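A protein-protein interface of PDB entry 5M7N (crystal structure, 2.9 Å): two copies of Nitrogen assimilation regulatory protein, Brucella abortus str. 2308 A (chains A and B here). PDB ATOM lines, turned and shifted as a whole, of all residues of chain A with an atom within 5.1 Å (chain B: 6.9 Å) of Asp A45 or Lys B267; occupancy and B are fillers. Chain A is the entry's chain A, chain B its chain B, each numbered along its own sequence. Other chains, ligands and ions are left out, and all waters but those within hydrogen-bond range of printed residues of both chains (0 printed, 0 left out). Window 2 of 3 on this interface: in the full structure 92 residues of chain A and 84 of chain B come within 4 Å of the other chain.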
ATOM      1  N   ARG A  31     -11.424  12.306 -26.016  1.00  0.00           N
ATOM      2  CA  ARG A  31     -11.124  13.509 -26.789  1.00  0.00           C
ATOM      3  C   ARG A  31      -9.645  13.427 -27.149  1.00  0.00           C
ATOM      4  O   ARG A  31      -8.864  12.897 -26.367  1.00  0.00           O
ATOM      5  CB  ARG A  31     -11.393  14.779 -25.980  1.00  0.00           C
ATOM      6  CG  ARG A  31     -12.845  14.930 -25.550  1.00  0.00           C
ATOM      7  CD  ARG A  31     -13.086  16.210 -24.767  1.00  0.00           C
ATOM      8  NE  ARG A  31     -12.622  16.100 -23.387  1.00  0.00           N
ATOM      9  CZ  ARG A  31     -12.289  17.133 -22.619  1.00  0.00           C
ATOM     10  NH1 ARG A  31     -12.357  18.370 -23.089  1.00  0.00           N
ATOM     11  NH2 ARG A  31     -11.878  16.936 -21.375  1.00  0.00           N
ATOM     12  N   ALA A  41      -6.211  23.483 -25.031  1.00  0.00           N
ATOM     13  CA  ALA A  41      -7.473  23.929 -25.620  1.00  0.00           C
ATOM     14  C   ALA A  41      -8.574  22.992 -25.134  1.00  0.00           C
ATOM     15  O   ALA A  41      -9.637  23.470 -24.757  1.00  0.00           O
ATOM     16  CB  ALA A  41      -7.390  23.885 -27.143  1.00  0.00           C
ATOM     17  N   ALA A  42      -8.306  21.669 -25.100  1.00  0.00           N
ATOM     18  CA  ALA A  42      -9.252  20.658 -24.628  1.00  0.00           C
ATOM     19  C   ALA A  42      -9.519  20.754 -23.121  1.00  0.00           C
ATOM     20  O   ALA A  42     -10.654  20.541 -22.704  1.00  0.00           O
ATOM     21  CB  ALA A  42      -8.751  19.277 -24.983  1.00  0.00           C
ATOM     22  N   ILE A  43      -8.480  21.079 -22.310  1.00  0.00           N
ATOM     23  CA  ILE A  43      -8.564  21.256 -20.850  1.00  0.00           C
ATOM     24  C   ILE A  43      -9.464  22.479 -20.587  1.00  0.00           C
ATOM     25  O   ILE A  43     -10.301  22.459 -19.672  1.00  0.00           O
ATOM     26  CB  ILE A  43      -7.161  21.449 -20.209  1.00  0.00           C
ATOM     27  CG1 ILE A  43      -6.138  20.333 -20.612  1.00  0.00           C
ATOM     28  CG2 ILE A  43      -7.253  21.619 -18.698  1.00  0.00           C
ATOM     29  CD1 ILE A  43      -6.238  18.933 -19.950  1.00  0.00           C
ATOM     30  N   ASN A  44      -9.290  23.532 -21.396  1.00  0.00           N
ATOM     31  CA  ASN A  44     -10.097  24.730 -21.302  1.00  0.00           C
ATOM     32  C   ASN A  44     -11.552  24.426 -21.644  1.00  0.00           C
ATOM     33  O   ASN A  44     -12.444  24.987 -21.007  1.00  0.00           O
ATOM     34  CB  ASN A  44      -9.557  25.813 -22.229  1.00  0.00           C
ATOM     35  CG  ASN A  44     -10.201  27.158 -22.025  1.00  0.00           C
ATOM     36  OD1 ASN A  44      -9.654  28.023 -21.341  1.00  0.00           O
ATOM     37  ND2 ASN A  44     -11.341  27.390 -22.665  1.00  0.00           N
ATOM     38  N   ASP A  45     -11.801  23.567 -22.663  1.00  0.00           N
ATOM     39  CA  ASP A  45     -13.156  23.205 -23.080  1.00  0.00           C
ATOM     40  C   ASP A  45     -13.901  22.603 -21.899  1.00  0.00           C
ATOM     41  O   ASP A  45     -15.054  22.974 -21.658  1.00  0.00           O
ATOM     42  CB  ASP A  45     -13.127  22.221 -24.267  1.00  0.00           C
ATOM     43  CG  ASP A  45     -12.652  22.789 -25.598  1.00  0.00           C
ATOM     44  OD1 ASP A  45     -12.293  23.996 -25.646  1.00  0.00           O
ATOM     45  OD2 ASP A  45     -12.630  22.028 -26.592  1.00  0.00           O
ATOM     46  N   ARG A  46     -13.212  21.712 -21.146  1.00  0.00           N
ATOM     47  CA  ARG A  46     -13.691  20.999 -19.957  1.00  0.00           C
ATOM     48  C   ARG A  46     -12.575  20.148 -19.393  1.00  0.00           C
ATOM     49  O   ARG A  46     -11.849  19.503 -20.150  1.00  0.00           O
ATOM     50  CB  ARG A  46     -14.881  20.083 -20.281  1.00  0.00           C
ATOM     51  CG  ARG A  46     -15.614  19.621 -19.041  1.00  0.00           C
ATOM     52  CD  ARG A  46     -16.830  18.829 -19.395  1.00  0.00           C
ATOM     53  NE  ARG A  46     -16.510  17.612 -20.139  1.00  0.00           N
ATOM     54  CZ  ARG A  46     -16.812  17.413 -21.414  1.00  0.00           C
ATOM     55  NH1 ARG A  46     -17.416  18.366 -22.114  1.00  0.00           N
ATOM     56  NH2 ARG A  46     -16.510  16.268 -22.005  1.00  0.00           N
ATOM     57  N   ALA A  47     -12.447  20.134 -18.066  1.00  0.00           N
ATOM     58  CA  ALA A  47     -11.393  19.375 -17.420  1.00  0.00           C
ATOM     59  C   ALA A  47     -11.720  17.886 -17.504  1.00  0.00           C
ATOM     60  O   ALA A  47     -12.847  17.478 -17.183  1.00  0.00           O
ATOM     61  CB  ALA A  47     -11.218  19.823 -15.980  1.00  0.00           C
ATOM     62  N   GLU B 216     -12.105  31.297 -15.250  1.00  0.00           N
ATOM     63  CA  GLU B 216     -11.218  31.042 -16.396  1.00  0.00           C
ATOM     64  C   GLU B 216      -9.723  31.174 -16.035  1.00  0.00           C
ATOM     65  O   GLU B 216      -9.397  31.788 -15.014  1.00  0.00           O
ATOM     66  CB  GLU B 216     -11.572  31.974 -17.561  1.00  0.00           C
ATOM     67  N   ARG B 222      -6.156  26.475 -11.498  1.00  0.00           N
ATOM     68  CA  ARG B 222      -7.495  26.612 -12.076  1.00  0.00           C
ATOM     69  C   ARG B 222      -8.604  26.257 -11.079  1.00  0.00           C
ATOM     70  O   ARG B 222      -8.519  25.214 -10.407  1.00  0.00           O
ATOM     71  CB  ARG B 222      -7.621  25.753 -13.345  1.00  0.00           C
ATOM     72  CG  ARG B 222      -8.737  26.200 -14.275  1.00  0.00           C
ATOM     73  CD  ARG B 222      -8.656  25.443 -15.573  1.00  0.00           C
ATOM     74  NE  ARG B 222      -9.276  26.181 -16.667  1.00  0.00           N
ATOM     75  CZ  ARG B 222      -8.804  26.214 -17.907  1.00  0.00           C
ATOM     76  NH1 ARG B 222      -7.700  25.541 -18.221  1.00  0.00           N
ATOM     77  NH2 ARG B 222      -9.422  26.920 -18.842  1.00  0.00           N
ATOM     78  N   GLU B 228     -18.853  21.393 -13.455  1.00  0.00           N
ATOM     79  CA  GLU B 228     -17.772  20.808 -14.238  1.00  0.00           C
ATOM     80  C   GLU B 228     -17.217  19.591 -13.497  1.00  0.00           C
ATOM     81  O   GLU B 228     -17.089  18.538 -14.105  1.00  0.00           O
ATOM     82  CB  GLU B 228     -16.681  21.852 -14.472  1.00  0.00           C
ATOM     83  CG  GLU B 228     -15.838  21.630 -15.711  1.00  0.00           C
ATOM     84  CD  GLU B 228     -14.742  22.660 -15.910  1.00  0.00           C
ATOM     85  OE1 GLU B 228     -14.773  23.722 -15.241  1.00  0.00           O
ATOM     86  OE2 GLU B 228     -13.857  22.410 -16.759  1.00  0.00           O
ATOM     87  N   GLN B 259     -25.351  23.394 -20.296  1.00  0.00           N
ATOM     88  CA  GLN B 259     -24.173  24.226 -20.559  1.00  0.00           C
ATOM     89  C   GLN B 259     -24.116  25.419 -19.627  1.00  0.00           C
ATOM     90  O   GLN B 259     -25.152  25.832 -19.086  1.00  0.00           O
ATOM     91  CB  GLN B 259     -24.162  24.742 -22.013  1.00  0.00           C
ATOM     92  CG  GLN B 259     -23.983  23.678 -23.083  1.00  0.00           C
ATOM     93  CD  GLN B 259     -23.635  24.307 -24.398  1.00  0.00           C
ATOM     94  OE1 GLN B 259     -22.472  24.623 -24.669  1.00  0.00           O
ATOM     95  NE2 GLN B 259     -24.642  24.533 -25.228  1.00  0.00           N
ATOM     96  N   PHE B 260     -22.916  26.007 -19.475  1.00  0.00           N
ATOM     97  CA  PHE B 260     -22.687  27.176 -18.619  1.00  0.00           C
ATOM     98  C   PHE B 260     -21.383  27.895 -18.975  1.00  0.00           C
ATOM     99  O   PHE B 260     -20.498  27.319 -19.603  1.00  0.00           O
ATOM    100  CB  PHE B 260     -22.689  26.782 -17.115  1.00  0.00           C
ATOM    101  CG  PHE B 260     -21.660  25.742 -16.725  1.00  0.00           C
ATOM    102  CD1 PHE B 260     -21.918  24.382 -16.894  1.00  0.00           C
ATOM    103  CD2 PHE B 260     -20.433  26.122 -16.191  1.00  0.00           C
ATOM    104  CE1 PHE B 260     -20.959  23.427 -16.562  1.00  0.00           C
ATOM    105  CE2 PHE B 260     -19.484  25.161 -15.835  1.00  0.00           C
ATOM    106  CZ  PHE B 260     -19.754  23.820 -16.025  1.00  0.00           C
ATOM    107  N   GLU B 261     -21.252  29.141 -18.528  1.00  0.00           N
ATOM    108  CA  GLU B 261     -20.038  29.920 -18.729  1.00  0.00           C
ATOM    109  C   GLU B 261     -19.278  30.001 -17.418  1.00  0.00           C
ATOM    110  O   GLU B 261     -19.890  30.004 -16.351  1.00  0.00           O
ATOM    111  CB  GLU B 261     -20.394  31.331 -19.191  1.00  0.00           C
ATOM    112  CG  GLU B 261     -20.942  31.364 -20.601  1.00  0.00           C
ATOM    113  CD  GLU B 261     -21.530  32.698 -21.003  1.00  0.00           C
ATOM    114  OE1 GLU B 261     -20.801  33.716 -20.932  1.00  0.00           O
ATOM    115  OE2 GLU B 261     -22.709  32.715 -21.425  1.00  0.00           O
ATOM    116  N   ARG B 262     -17.964  30.096 -17.485  1.00  0.00           N
ATOM    117  CA  ARG B 262     -17.179  30.261 -16.275  1.00  0.00           C
ATOM    118  C   ARG B 262     -17.084  31.762 -15.984  1.00  0.00           C
ATOM    119  O   ARG B 262     -17.096  32.569 -16.920  1.00  0.00           O
ATOM    120  CB  ARG B 262     -15.770  29.682 -16.450  1.00  0.00           C
ATOM    121  CG  ARG B 262     -15.717  28.186 -16.682  1.00  0.00           C
ATOM    122  CD  ARG B 262     -14.285  27.717 -16.661  1.00  0.00           C
ATOM    123  NE  ARG B 262     -14.176  26.316 -17.056  1.00  0.00           N
ATOM    124  CZ  ARG B 262     -13.562  25.898 -18.154  1.00  0.00           C
ATOM    125  NH1 ARG B 262     -12.973  26.764 -18.965  1.00  0.00           N
ATOM    126  NH2 ARG B 262     -13.514  24.604 -18.441  1.00  0.00           N
ATOM    127  N   VAL B 263     -16.974  32.129 -14.698  1.00  0.00           N
ATOM    128  CA  VAL B 263     -16.839  33.517 -14.241  1.00  0.00           C
ATOM    129  C   VAL B 263     -15.588  34.166 -14.872  1.00  0.00           C
ATOM    130  O   VAL B 263     -14.526  33.540 -14.907  1.00  0.00           O
ATOM    131  CB  VAL B 263     -16.877  33.592 -12.689  1.00  0.00           C
ATOM    132  CG1 VAL B 263     -16.440  34.961 -12.158  1.00  0.00           C
ATOM    133  CG2 VAL B 263     -18.264  33.222 -12.164  1.00  0.00           C
ATOM    134  N   GLY B 265     -15.133  34.709 -18.049  1.00  0.00           N
ATOM    135  CA  GLY B 265     -14.802  33.952 -19.251  1.00  0.00           C
ATOM    136  C   GLY B 265     -15.931  33.750 -20.238  1.00  0.00           C
ATOM    137  O   GLY B 265     -17.084  33.552 -19.843  1.00  0.00           O
ATOM    138  N   THR B 266     -15.571  33.797 -21.544  1.00  0.00           N
ATOM    139  CA  THR B 266     -16.447  33.613 -22.719  1.00  0.00           C
ATOM    140  C   THR B 266     -16.825  32.126 -22.927  1.00  0.00           C
ATOM    141  O   THR B 266     -17.949  31.846 -23.356  1.00  0.00           O
ATOM    142  CB  THR B 266     -15.787  34.214 -24.010  1.00  0.00           C
ATOM    143  OG1 THR B 266     -16.560  33.882 -25.173  1.00  0.00           O
ATOM    144  CG2 THR B 266     -14.326  33.743 -24.222  1.00  0.00           C
ATOM    145  N   LYS B 267     -15.867  31.197 -22.650  1.00  0.00           N
ATOM    146  CA  LYS B 267     -16.011  29.761 -22.850  1.00  0.00           C
ATOM    147  C   LYS B 267     -17.244  29.176 -22.167  1.00  0.00           C
ATOM    148  O   LYS B 267     -17.540  29.432 -20.993  1.00  0.00           O
ATOM    149  CB  LYS B 267     -14.744  28.953 -22.510  1.00  0.00           C
ATOM    150  CG  LYS B 267     -14.736  27.519 -23.086  1.00  0.00           C
ATOM    151  CD  LYS B 267     -14.318  27.470 -24.563  1.00  0.00           C
ATOM    152  CE  LYS B 267     -14.371  26.094 -25.169  1.00  0.00           C
ATOM    153  NZ  LYS B 267     -15.756  25.641 -25.467  1.00  0.00           N
ATOM    154  N   ARG B 268     -17.984  28.418 -22.981  1.00  0.00           N
ATOM    155  CA  ARG B 268     -19.207  27.714 -22.632  1.00  0.00           C
ATOM    156  C   ARG B 268     -18.926  26.214 -22.562  1.00  0.00           C
ATOM    157  O   ARG B 268     -18.465  25.599 -23.530  1.00  0.00           O
ATOM    158  CB  ARG B 268     -20.302  28.084 -23.635  1.00  0.00           C
ATOM    159  CG  ARG B 268     -21.612  28.298 -22.931  1.00  0.00           C
ATOM    160  CD  ARG B 268     -22.620  28.989 -23.806  1.00  0.00           C
ATOM    161  NE  ARG B 268     -23.971  28.667 -23.343  1.00  0.00           N
ATOM    162  CZ  ARG B 268     -24.580  29.260 -22.315  1.00  0.00           C
ATOM    163  NH1 ARG B 268     -23.974  30.232 -21.640  1.00  0.00           N
ATOM    164  NH2 ARG B 268     -25.804  28.886 -21.959  1.00  0.00           N
ATOM    165  N   VAL B 269     -19.130  25.651 -21.365  1.00  0.00           N
ATOM    166  CA  VAL B 269     -18.857  24.262 -21.004  1.00  0.00           C
ATOM    167  C   VAL B 269     -20.140  23.415 -20.988  1.00  0.00           C
ATOM    168  O   VAL B 269     -21.152  23.842 -20.421  1.00  0.00           O
ATOM    169  CB  VAL B 269     -18.123  24.173 -19.620  1.00  0.00           C
ATOM    170  CG1 VAL B 269     -17.654  22.758 -19.320  1.00  0.00           C
ATOM    171  CG2 VAL B 269     -16.957  25.156 -19.521  1.00  0.00           C
ATOM    172  N   LYS B 270     -20.079  22.216 -21.596  1.00  0.00           N
ATOM    173  CA  LYS B 270     -21.182  21.264 -21.564  1.00  0.00           C
ATOM    174  C   LYS B 270     -20.768  20.081 -20.676  1.00  0.00           C
ATOM    175  O   LYS B 270     -19.689  19.500 -20.859  1.00  0.00           O
ATOM    176  CB  LYS B 270     -21.643  20.801 -22.963  1.00  0.00           C
ATOM    177  CG  LYS B 270     -22.969  20.018 -22.902  1.00  0.00           C
ATOM    178  CD  LYS B 270     -23.469  19.595 -24.264  1.00  0.00           C
ATOM    179  CE  LYS B 270     -24.789  18.872 -24.157  1.00  0.00           C
ATOM    180  NZ  LYS B 270     -25.216  18.312 -25.467  1.00  0.00           N
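OD1 of Asn A44 lies within hydrogen-bond range of NH2 of Arg B222 (2.7 Å). NH1 of Arg B262 lies within hydrogen-bond range of O of Asn A44 (2.8 Å). OD1 of Asp A45 lies within salt-bridge range of NZ of Lys B267 (3.8 Å). The backbone carbonyl oxygen of Lys B270 is in hydrogen-bond range of the guanidinium group of Arg A46, at 2.8 Å. OE2 of Glu B228 is in hydrogen-bond range of N of Ala A47 (3.0 Å).
The guanidinium group (NH2) of Arg A31 sits at hydrogen-bond distance from the backbone carbonyl oxygen (O) of Arg A46 (2.8 Å). OE2 of Glu B228 lies within salt-bridge range of NH2 of Arg B262 (2.8 Å). The backbone carbonyl oxygen of Phe B260 is in hydrogen-bond range of the backbone NH of Val B269, at 2.8 Å.
Ile A43 touches Arg B222. Asn A44 touches Lys B267 (ND2 to CG, 3.4 Å). Asp A45 touches Arg B262 (O to NH2, 3.9 Å). Asp A45 touches Val B269. CA of Arg A46 touches OE2 of Glu B228, at 3.5 Å. CA of Arg A46 touches NH2 of Arg B262 (3.9 Å). Arg A46 touches Val B269.
Asp A45 touches just these residues of chain B: Arg B262 (3.9 Å), Lys B267 (3.0 Å) and Val B269 (3.5 Å). Of the printed residues of chain B, Ala A47 touches Glu B228. Glu B216 touches none of the printed residues of chain A. Of the printed residues of chain A, Arg B222 touches Ile A43 (3.98 Å) and Asn A44 (2.7 Å). Lys B267 touches two residues of chain A. Printed residues of chain A within 4 Å of Val B269: Asp A45 and Arg A46. The nearest printed residue of chain A that does not touch Lys B267 is Ala A41 (5.4 Å).
Printed residues of chain A that touch a printed residue of chain B: Ile A43, Asn A44, Asp A45, Arg A46 and Ala A47. Hydrophobic or aromatic side chains of chain A that line the printed part of chain B: Ile A43 and Ala A47. Of the 14 printed residues of chain B, 6 touch a printed residue of chain A. Among the printed residues, 12 pairs touch across the chains.
No position is printed for both chains. Of the 12 pairs that touch across the chains among the printed residues, none has its exchanged pair printed and touching as well.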
